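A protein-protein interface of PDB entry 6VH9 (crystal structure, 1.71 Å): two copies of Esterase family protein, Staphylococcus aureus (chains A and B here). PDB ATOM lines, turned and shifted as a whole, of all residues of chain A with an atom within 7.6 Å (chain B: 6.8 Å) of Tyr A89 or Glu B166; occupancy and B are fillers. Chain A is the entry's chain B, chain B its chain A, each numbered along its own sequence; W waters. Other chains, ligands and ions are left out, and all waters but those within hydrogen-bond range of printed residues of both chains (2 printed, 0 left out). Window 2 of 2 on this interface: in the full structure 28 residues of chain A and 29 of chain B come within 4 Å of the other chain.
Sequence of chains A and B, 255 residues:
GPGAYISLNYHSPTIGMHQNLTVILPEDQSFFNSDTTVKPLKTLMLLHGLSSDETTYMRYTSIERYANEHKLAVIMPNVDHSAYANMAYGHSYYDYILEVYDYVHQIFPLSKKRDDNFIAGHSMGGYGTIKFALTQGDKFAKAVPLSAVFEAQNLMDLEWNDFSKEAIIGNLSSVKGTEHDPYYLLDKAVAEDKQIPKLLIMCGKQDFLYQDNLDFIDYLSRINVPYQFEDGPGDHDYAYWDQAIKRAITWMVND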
ATOM      1  N   ASN A  86       0.842 -32.449 -21.830  1.00  0.00           N
ATOM      2  CA  ASN A  86       1.515 -32.996 -23.006  1.00  0.00           C
ATOM      3  C   ASN A  86       2.474 -31.920 -23.509  1.00  0.00           C
ATOM      4  O   ASN A  86       2.059 -30.929 -24.124  1.00  0.00           O
ATOM      5  CB  ASN A  86       0.510 -33.411 -24.079  1.00  0.00           C
ATOM      6  CG  ASN A  86      -0.310 -34.629 -23.666  1.00  0.00           C
ATOM      7  OD1 ASN A  86       0.159 -35.479 -22.910  1.00  0.00           O
ATOM      8  ND2 ASN A  86      -1.537 -34.714 -24.157  1.00  0.00           N
ATOM      9  N   MET A  87       3.770 -32.109 -23.244  1.00  0.00           N
ATOM     10  CA  MET A  87       4.736 -31.028 -23.370  1.00  0.00           C
ATOM     11  C   MET A  87       5.040 -30.702 -24.829  1.00  0.00           C
ATOM     12  O   MET A  87       5.151 -31.595 -25.674  1.00  0.00           O
ATOM     13  CB  MET A  87       6.034 -31.388 -22.645  1.00  0.00           C
ATOM     14  CG  MET A  87       5.865 -31.606 -21.147  1.00  0.00           C
ATOM     15  SD  MET A  87       7.321 -32.360 -20.386  1.00  0.00           S
ATOM     16  CE  MET A  87       8.458 -30.988 -20.318  1.00  0.00           C
ATOM     17  N   ALA A  88       5.210 -29.404 -25.112  1.00  0.00           N
ATOM     18  CA  ALA A  88       5.624 -28.989 -26.449  1.00  0.00           C
ATOM     19  C   ALA A  88       6.941 -29.648 -26.852  1.00  0.00           C
ATOM     20  O   ALA A  88       7.073 -30.162 -27.967  1.00  0.00           O
ATOM     21  CB  ALA A  88       5.743 -27.462 -26.520  1.00  0.00           C
ATOM     22  N   TYR A  89       7.939 -29.621 -25.964  1.00  0.00           N
ATOM     23  CA  TYR A  89       9.240 -30.264 -26.183  1.00  0.00           C
ATOM     24  C   TYR A  89       9.531 -31.151 -24.972  1.00  0.00           C
ATOM     25  O   TYR A  89      10.167 -30.717 -24.007  1.00  0.00           O
ATOM     26  CB  TYR A  89      10.338 -29.244 -26.384  1.00  0.00           C
ATOM     27  CG  TYR A  89      10.051 -28.251 -27.485  1.00  0.00           C
ATOM     28  CD1 TYR A  89       9.823 -26.918 -27.195  1.00  0.00           C
ATOM     29  CD2 TYR A  89       9.997 -28.659 -28.810  1.00  0.00           C
ATOM     30  CE1 TYR A  89       9.566 -26.000 -28.211  1.00  0.00           C
ATOM     31  CE2 TYR A  89       9.746 -27.752 -29.835  1.00  0.00           C
ATOM     32  CZ  TYR A  89       9.526 -26.429 -29.524  1.00  0.00           C
ATOM     33  OH  TYR A  89       9.274 -25.527 -30.529  1.00  0.00           O
ATOM     34  N   GLY A  90       9.075 -32.397 -25.021  1.00  0.00           N
ATOM     35  CA  GLY A  90       9.239 -33.269 -23.874  1.00  0.00           C
ATOM     36  C   GLY A  90       8.326 -34.465 -23.993  1.00  0.00           C
ATOM     37  O   GLY A  90       8.183 -35.019 -25.086  1.00  0.00           O
ATOM     38  N   HIS A  91       7.703 -34.872 -22.892  1.00  0.00           N
ATOM     39  CA  HIS A  91       6.887 -36.076 -22.836  1.00  0.00           C
ATOM     40  C   HIS A  91       5.400 -35.752 -22.800  1.00  0.00           C
ATOM     41  O   HIS A  91       4.979 -34.647 -22.430  1.00  0.00           O
ATOM     42  CB  HIS A  91       7.229 -36.918 -21.596  1.00  0.00           C
ATOM     43  CG  HIS A  91       8.596 -37.521 -21.623  1.00  0.00           C
ATOM     44  ND1 HIS A  91       8.888 -38.675 -22.323  1.00  0.00           N
ATOM     45  CD2 HIS A  91       9.744 -37.157 -21.000  1.00  0.00           C
ATOM     46  CE1 HIS A  91      10.160 -38.989 -22.141  1.00  0.00           C
ATOM     47  NE2 HIS A  91      10.705 -38.078 -21.352  1.00  0.00           N
ATOM     48  N   SER A 164      12.003 -25.484 -16.992  1.00  0.00           N
ATOM     49  CA  SER A 164      11.862 -24.921 -18.335  1.00  0.00           C
ATOM     50  C   SER A 164      10.389 -24.705 -18.676  1.00  0.00           C
ATOM     51  O   SER A 164       9.656 -25.666 -18.953  1.00  0.00           O
ATOM     52  CB  SER A 164      12.518 -25.827 -19.375  1.00  0.00           C
ATOM     53  OG  SER A 164      12.222 -25.336 -20.673  1.00  0.00           O
ATOM     54  N   LYS A 165       9.964 -23.439 -18.720  1.00  0.00           N
ATOM     55  CA  LYS A 165       8.588 -23.184 -19.131  1.00  0.00           C
ATOM     56  C   LYS A 165       8.388 -23.499 -20.609  1.00  0.00           C
ATOM     57  O   LYS A 165       7.321 -23.988 -20.993  1.00  0.00           O
ATOM     58  CB  LYS A 165       8.179 -21.740 -18.805  1.00  0.00           C
ATOM     59  CG  LYS A 165       8.266 -20.745 -19.935  1.00  0.00           C
ATOM     60  CD  LYS A 165       7.621 -19.421 -19.527  1.00  0.00           C
ATOM     61  CE  LYS A 165       8.508 -18.240 -19.882  1.00  0.00           C
ATOM     62  NZ  LYS A 165       7.834 -16.935 -19.599  1.00  0.00           N
ATOM     63  N   GLU A 166       9.402 -23.252 -21.451  1.00  0.00           N
ATOM     64  CA  GLU A 166       9.232 -23.485 -22.886  1.00  0.00           C
ATOM     65  C   GLU A 166       9.129 -24.972 -23.217  1.00  0.00           C
ATOM     66  O   GLU A 166       8.498 -25.333 -24.214  1.00  0.00           O
ATOM     67  CB  GLU A 166      10.382 -22.859 -23.675  1.00  0.00           C
ATOM     68  CG  GLU A 166      10.387 -21.341 -23.678  1.00  0.00           C
ATOM     69  CD  GLU A 166      11.121 -20.748 -22.482  1.00  0.00           C
ATOM     70  OE1 GLU A 166      11.673 -21.519 -21.663  1.00  0.00           O
ATOM     71  OE2 GLU A 166      11.152 -19.503 -22.363  1.00  0.00           O
ATOM     72  N   ALA A 167       9.738 -25.849 -22.406  1.00  0.00           N
ATOM     73  CA  ALA A 167       9.533 -27.281 -22.621  1.00  0.00           C
ATOM     74  C   ALA A 167       8.052 -27.625 -22.574  1.00  0.00           C
ATOM     75  O   ALA A 167       7.574 -28.467 -23.346  1.00  0.00           O
ATOM     76  CB  ALA A 167      10.293 -28.100 -21.577  1.00  0.00           C
ATOM     77  N   ILE A 168       7.305 -26.961 -21.694  1.00  0.00           N
ATOM     78  CA  ILE A 168       5.882 -27.236 -21.540  1.00  0.00           C
ATOM     79  C   ILE A 168       5.072 -26.541 -22.631  1.00  0.00           C
ATOM     80  O   ILE A 168       4.281 -27.168 -23.349  1.00  0.00           O
ATOM     81  CB  ILE A 168       5.406 -26.794 -20.145  1.00  0.00           C
ATOM     82  CG1 ILE A 168       6.166 -27.532 -19.044  1.00  0.00           C
ATOM     83  CG2 ILE A 168       3.924 -27.031 -20.003  1.00  0.00           C
ATOM     84  CD1 ILE A 168       5.967 -26.910 -17.681  1.00  0.00           C
ATOM     85  N   ILE A 169       5.200 -25.214 -22.731  1.00  0.00           N
ATOM     86  CA  ILE A 169       4.273 -24.439 -23.548  1.00  0.00           C
ATOM     87  C   ILE A 169       4.854 -24.024 -24.896  1.00  0.00           C
ATOM     88  O   ILE A 169       4.147 -23.386 -25.684  1.00  0.00           O
ATOM     89  CB  ILE A 169       3.750 -23.197 -22.796  1.00  0.00           C
ATOM     90  CG1 ILE A 169       4.867 -22.177 -22.586  1.00  0.00           C
ATOM     91  CG2 ILE A 169       3.109 -23.611 -21.482  1.00  0.00           C
ATOM     92  CD1 ILE A 169       4.369 -20.859 -21.998  1.00  0.00           C
ATOM     93  N   GLY A 170       6.107 -24.353 -25.181  1.00  0.00           N
ATOM     94  CA  GLY A 170       6.687 -23.974 -26.458  1.00  0.00           C
ATOM     95  C   GLY A 170       6.903 -22.474 -26.509  1.00  0.00           C
ATOM     96  O   GLY A 170       7.336 -21.857 -25.528  1.00  0.00           O
ATOM     97  N   ASN A 171       6.570 -21.871 -27.646  1.00  0.00           N
ATOM     98  CA  ASN A 171       6.825 -20.455 -27.893  1.00  0.00           C
ATOM     99  C   ASN A 171       5.733 -19.537 -27.358  1.00  0.00           C
ATOM    100  O   ASN A 171       5.828 -18.319 -27.548  1.00  0.00           O
ATOM    101  CB  ASN A 171       6.991 -20.216 -29.395  1.00  0.00           C
ATOM    102  CG  ASN A 171       5.932 -20.923 -30.200  1.00  0.00           C
ATOM    103  OD1 ASN A 171       6.021 -22.128 -30.439  1.00  0.00           O
ATOM    104  ND2 ASN A 171       4.903 -20.188 -30.601  1.00  0.00           N
ATOM    105  N   MET B  87      19.988 -29.709 -21.668  1.00  0.00           N
ATOM    106  CA  MET B  87      18.964 -29.642 -22.694  1.00  0.00           C
ATOM    107  C   MET B  87      18.562 -28.203 -22.998  1.00  0.00           C
ATOM    108  O   MET B  87      18.447 -27.362 -22.100  1.00  0.00           O
ATOM    109  CB  MET B  87      17.745 -30.447 -22.249  1.00  0.00           C
ATOM    110  CG  MET B  87      18.040 -31.952 -22.073  1.00  0.00           C
ATOM    111  SD  MET B  87      16.650 -32.802 -21.291  1.00  0.00           S
ATOM    112  CE  MET B  87      15.422 -32.646 -22.600  1.00  0.00           C
ATOM    113  N   ALA B  88      18.331 -27.936 -24.282  1.00  0.00           N
ATOM    114  CA  ALA B  88      17.822 -26.631 -24.703  1.00  0.00           C
ATOM    115  C   ALA B  88      16.526 -26.288 -23.976  1.00  0.00           C
ATOM    116  O   ALA B  88      16.378 -25.190 -23.429  1.00  0.00           O
ATOM    117  CB  ALA B  88      17.622 -26.628 -26.219  1.00  0.00           C
ATOM    118  N   TYR B  89      15.579 -27.228 -23.946  1.00  0.00           N
ATOM    119  CA  TYR B  89      14.317 -27.101 -23.210  1.00  0.00           C
ATOM    120  C   TYR B  89      14.168 -28.340 -22.324  1.00  0.00           C
ATOM    121  O   TYR B  89      13.603 -29.353 -22.741  1.00  0.00           O
ATOM    122  CB  TYR B  89      13.131 -26.955 -24.149  1.00  0.00           C
ATOM    123  CG  TYR B  89      13.338 -25.902 -25.201  1.00  0.00           C
ATOM    124  CD1 TYR B  89      13.413 -26.240 -26.540  1.00  0.00           C
ATOM    125  CD2 TYR B  89      13.482 -24.568 -24.843  1.00  0.00           C
ATOM    126  CE1 TYR B  89      13.610 -25.256 -27.517  1.00  0.00           C
ATOM    127  CE2 TYR B  89      13.682 -23.584 -25.806  1.00  0.00           C
ATOM    128  CZ  TYR B  89      13.746 -23.936 -27.135  1.00  0.00           C
ATOM    129  OH  TYR B  89      13.940 -22.953 -28.081  1.00  0.00           O
ATOM    130  N   GLY B  90      14.682 -28.268 -21.104  1.00  0.00           N
ATOM    131  CA  GLY B  90      14.629 -29.414 -20.220  1.00  0.00           C
ATOM    132  C   GLY B  90      15.584 -29.252 -19.063  1.00  0.00           C
ATOM    133  O   GLY B  90      15.748 -28.144 -18.540  1.00  0.00           O
ATOM    134  N   MET B 156      19.519 -38.075 -32.904  1.00  0.00           N
ATOM    135  CA  MET B 156      18.566 -36.970 -32.907  1.00  0.00           C
ATOM    136  C   MET B 156      17.412 -37.201 -33.877  1.00  0.00           C
ATOM    137  O   MET B 156      16.281 -36.798 -33.589  1.00  0.00           O
ATOM    138  CB  MET B 156      19.282 -35.652 -33.221  1.00  0.00           C
ATOM    139  CG  MET B 156      20.383 -35.261 -32.233  1.00  0.00           C
ATOM    140  SD  MET B 156      19.854 -35.402 -30.510  1.00  0.00           S
ATOM    141  CE  MET B 156      21.388 -35.119 -29.625  1.00  0.00           C
ATOM    142  N   PHE B 163       9.971 -39.289 -27.995  1.00  0.00           N
ATOM    143  CA  PHE B 163      11.286 -38.663 -27.907  1.00  0.00           C
ATOM    144  C   PHE B 163      11.270 -37.306 -28.605  1.00  0.00           C
ATOM    145  O   PHE B 163      10.759 -37.192 -29.719  1.00  0.00           O
ATOM    146  CB  PHE B 163      12.325 -39.574 -28.557  1.00  0.00           C
ATOM    147  CG  PHE B 163      13.687 -38.961 -28.679  1.00  0.00           C
ATOM    148  CD1 PHE B 163      14.487 -38.798 -27.556  1.00  0.00           C
ATOM    149  CD2 PHE B 163      14.195 -38.597 -29.915  1.00  0.00           C
ATOM    150  CE1 PHE B 163      15.752 -38.240 -27.665  1.00  0.00           C
ATOM    151  CE2 PHE B 163      15.457 -38.045 -30.028  1.00  0.00           C
ATOM    152  CZ  PHE B 163      16.239 -37.866 -28.898  1.00  0.00           C
ATOM    153  N   SER B 164      11.840 -36.275 -27.970  1.00  0.00           N
ATOM    154  CA  SER B 164      11.847 -34.927 -28.547  1.00  0.00           C
ATOM    155  C   SER B 164      13.281 -34.497 -28.839  1.00  0.00           C
ATOM    156  O   SER B 164      14.050 -34.193 -27.920  1.00  0.00           O
ATOM    157  CB  SER B 164      11.162 -33.915 -27.632  1.00  0.00           C
ATOM    158  OG  SER B 164      11.460 -32.581 -28.068  1.00  0.00           O
ATOM    159  N   LYS B 165      13.626 -34.414 -30.127  1.00  0.00           N
ATOM    160  CA  LYS B 165      14.962 -33.957 -30.476  1.00  0.00           C
ATOM    161  C   LYS B 165      15.131 -32.473 -30.151  1.00  0.00           C
ATOM    162  O   LYS B 165      16.189 -32.054 -29.665  1.00  0.00           O
ATOM    163  CB  LYS B 165      15.231 -34.283 -31.943  1.00  0.00           C
ATOM    164  CG  LYS B 165      16.018 -33.282 -32.728  1.00  0.00           C
ATOM    165  CD  LYS B 165      15.996 -33.667 -34.198  1.00  0.00           C
ATOM    166  CE  LYS B 165      14.725 -33.213 -34.881  1.00  0.00           C
ATOM    167  NZ  LYS B 165      14.934 -31.910 -35.553  1.00  0.00           N
ATOM    168  N   GLU B 166      14.070 -31.667 -30.337  1.00  0.00           N
ATOM    169  CA  GLU B 166      14.175 -30.232 -30.067  1.00  0.00           C
ATOM    170  C   GLU B 166      14.331 -29.934 -28.579  1.00  0.00           C
ATOM    171  O   GLU B 166      14.913 -28.907 -28.219  1.00  0.00           O
ATOM    172  CB  GLU B 166      12.945 -29.506 -30.609  1.00  0.00           C
ATOM    173  CG  GLU B 166      12.868 -29.471 -32.123  1.00  0.00           C
ATOM    174  CD  GLU B 166      12.235 -30.721 -32.713  1.00  0.00           C
ATOM    175  OE1 GLU B 166      11.879 -31.644 -31.942  1.00  0.00           O
ATOM    176  OE2 GLU B 166      12.096 -30.778 -33.954  1.00  0.00           O
ATOM    177  N   ALA B 167      13.808 -30.793 -27.700  1.00  0.00           N
ATOM    178  CA  ALA B 167      14.061 -30.599 -26.274  1.00  0.00           C
ATOM    179  C   ALA B 167      15.560 -30.579 -25.984  1.00  0.00           C
ATOM    180  O   ALA B 167      16.030 -29.823 -25.125  1.00  0.00           O
ATOM    181  CB  ALA B 167      13.368 -31.695 -25.454  1.00  0.00           C
ATOM    182  N   ILE B 168      16.326 -31.385 -26.713  1.00  0.00           N
ATOM    183  CA  ILE B 168      17.765 -31.461 -26.500  1.00  0.00           C
ATOM    184  C   ILE B 168      18.478 -30.304 -27.184  1.00  0.00           C
ATOM    185  O   ILE B 168      19.229 -29.554 -26.552  1.00  0.00           O
ATOM    186  CB  ILE B 168      18.309 -32.805 -27.008  1.00  0.00           C
ATOM    187  CG1 ILE B 168      17.691 -33.960 -26.206  1.00  0.00           C
ATOM    188  CG2 ILE B 168      19.835 -32.828 -26.925  1.00  0.00           C
ATOM    189  CD1 ILE B 168      17.967 -35.299 -26.812  1.00  0.00           C
ATOM    190  N   ILE B 169      18.311 -30.209 -28.494  1.00  0.00           N
ATOM    191  CA  ILE B 169      19.163 -29.289 -29.299  1.00  0.00           C
ATOM    192  C   ILE B 169      18.474 -27.976 -29.648  1.00  0.00           C
ATOM    193  O   ILE B 169      19.140 -27.117 -30.204  1.00  0.00           O
ATOM    194  CB  ILE B 169      19.603 -30.003 -30.582  1.00  0.00           C
ATOM    195  CG1 ILE B 169      18.401 -30.254 -31.488  1.00  0.00           C
ATOM    196  CG2 ILE B 169      20.331 -31.287 -30.267  1.00  0.00           C
ATOM    197  CD1 ILE B 169      18.736 -30.934 -32.765  1.00  0.00           C
ATOM    198  N   GLY B 170      17.211 -27.826 -29.299  1.00  0.00           N
ATOM    199  CA  GLY B 170      16.496 -26.593 -29.635  1.00  0.00           C
ATOM    200  C   GLY B 170      16.326 -26.388 -31.123  1.00  0.00           C
ATOM    201  O   GLY B 170      15.932 -27.309 -31.791  1.00  0.00           O
ATOM    202  N   ASN B 171      16.650 -25.207 -31.632  1.00  0.00           N
ATOM    203  CA  ASN B 171      16.340 -24.939 -33.063  1.00  0.00           C
ATOM    204  C   ASN B 171      17.494 -25.284 -34.005  1.00  0.00           C
ATOM    205  O   ASN B 171      17.349 -24.994 -35.185  1.00  0.00           O
ATOM    206  CB  ASN B 171      15.863 -23.503 -33.272  1.00  0.00           C
ATOM    207  CG  ASN B 171      16.983 -22.495 -33.246  1.00  0.00           C
ATOM    208  OD1 ASN B 171      18.144 -22.845 -33.089  1.00  0.00           O
ATOM    209  ND2 ASN B 171      16.642 -21.232 -33.432  1.00  0.00           N
HETATM  210  O   HOH W   1      11.916 -31.341 -22.053  1.00  0.00           O
HETATM  211  O   HOH W   2      11.033 -36.898 -24.857  1.00  0.00           O
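Among the printed residues, merely in contact across the chains: Tyr A89 with Glu B166, Tyr A89 with Ala B167, Gly A90 with Ser B164, Ser A164 with Gly B90, Tyr A89 with Tyr B89, Tyr A89 with Ser B164, Ala A167 with Tyr B89, Glu A166 with Tyr B89 and Ser A164 with Tyr B89.
Tyr A89 touches just these residues of chain B: Tyr B89, Ser B164, Glu B166 and Ala B167. Of the printed residues of chain A, Ser B164 touches Tyr A89 and Gly A90. Of the printed residues of chain B, Ala A167 touches Tyr B89. Gly A170 touches none of the printed residues of chain B. Phe B163 touches none of the printed residues of chain A. The nearest residue of chain B that does not touch Tyr A89 is Met B87 (5.8 Å). The nearest residue of chain A that does not touch Glu B166 is Ala A88 (6.4 Å).
The backbone carbonyl oxygen (O) of Ala B167 sits at hydrogen-bond distance from the backbone NH (N) of Tyr B89 (2.9 Å). The backbone NH of Ala A167 is in hydrogen-bond range of the side-chain hydroxyl of Ser A164 (3.1 Å). N of Ala A88 is in hydrogen-bond range of O of Ala A167, at 3.1 Å. O of Ala B167 lies within hydrogen-bond range of N of Ala B88 (3.1 Å). OG of Ser B164 lies within hydrogen-bond range of N of Ala B167, at 3.0 Å. N of Tyr A89 sits at hydrogen-bond distance from O of Ala A167, 2.9 Å away.
Water W1 lies within hydrogen-bond range of O of Tyr A89 (2.7 Å) and O of Tyr B89 (2.7 Å). Water W2 bridges N of Ser B164 (3.3 Å) and O of Gly A90 (3.4 Å).
Tyr A89 touches Ser B164, and with the chains exchanged Ser A164 touches Tyr B89. Tyr A89 touches Glu B166, and with the chains exchanged Glu A166 touches Tyr B89. Tyr A89 touches Ala B167, and with the chains exchanged Ala A167 touches Tyr B89. Gly A90 touches Ser B164, and with the chains exchanged Ser A164 touches Gly B90.
Hydrophobic or aromatic side chains of chain B within 4 Å of the printed part of chain A: Tyr B89 and Ala B167. Along chain B the printed residues that touch a printed residue of chain A span positions 89 to 167. Among the printed residues, no Asp or Glu carboxylate lies within 4 Å of a Lys or Arg side-chain nitrogen of the other chain.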
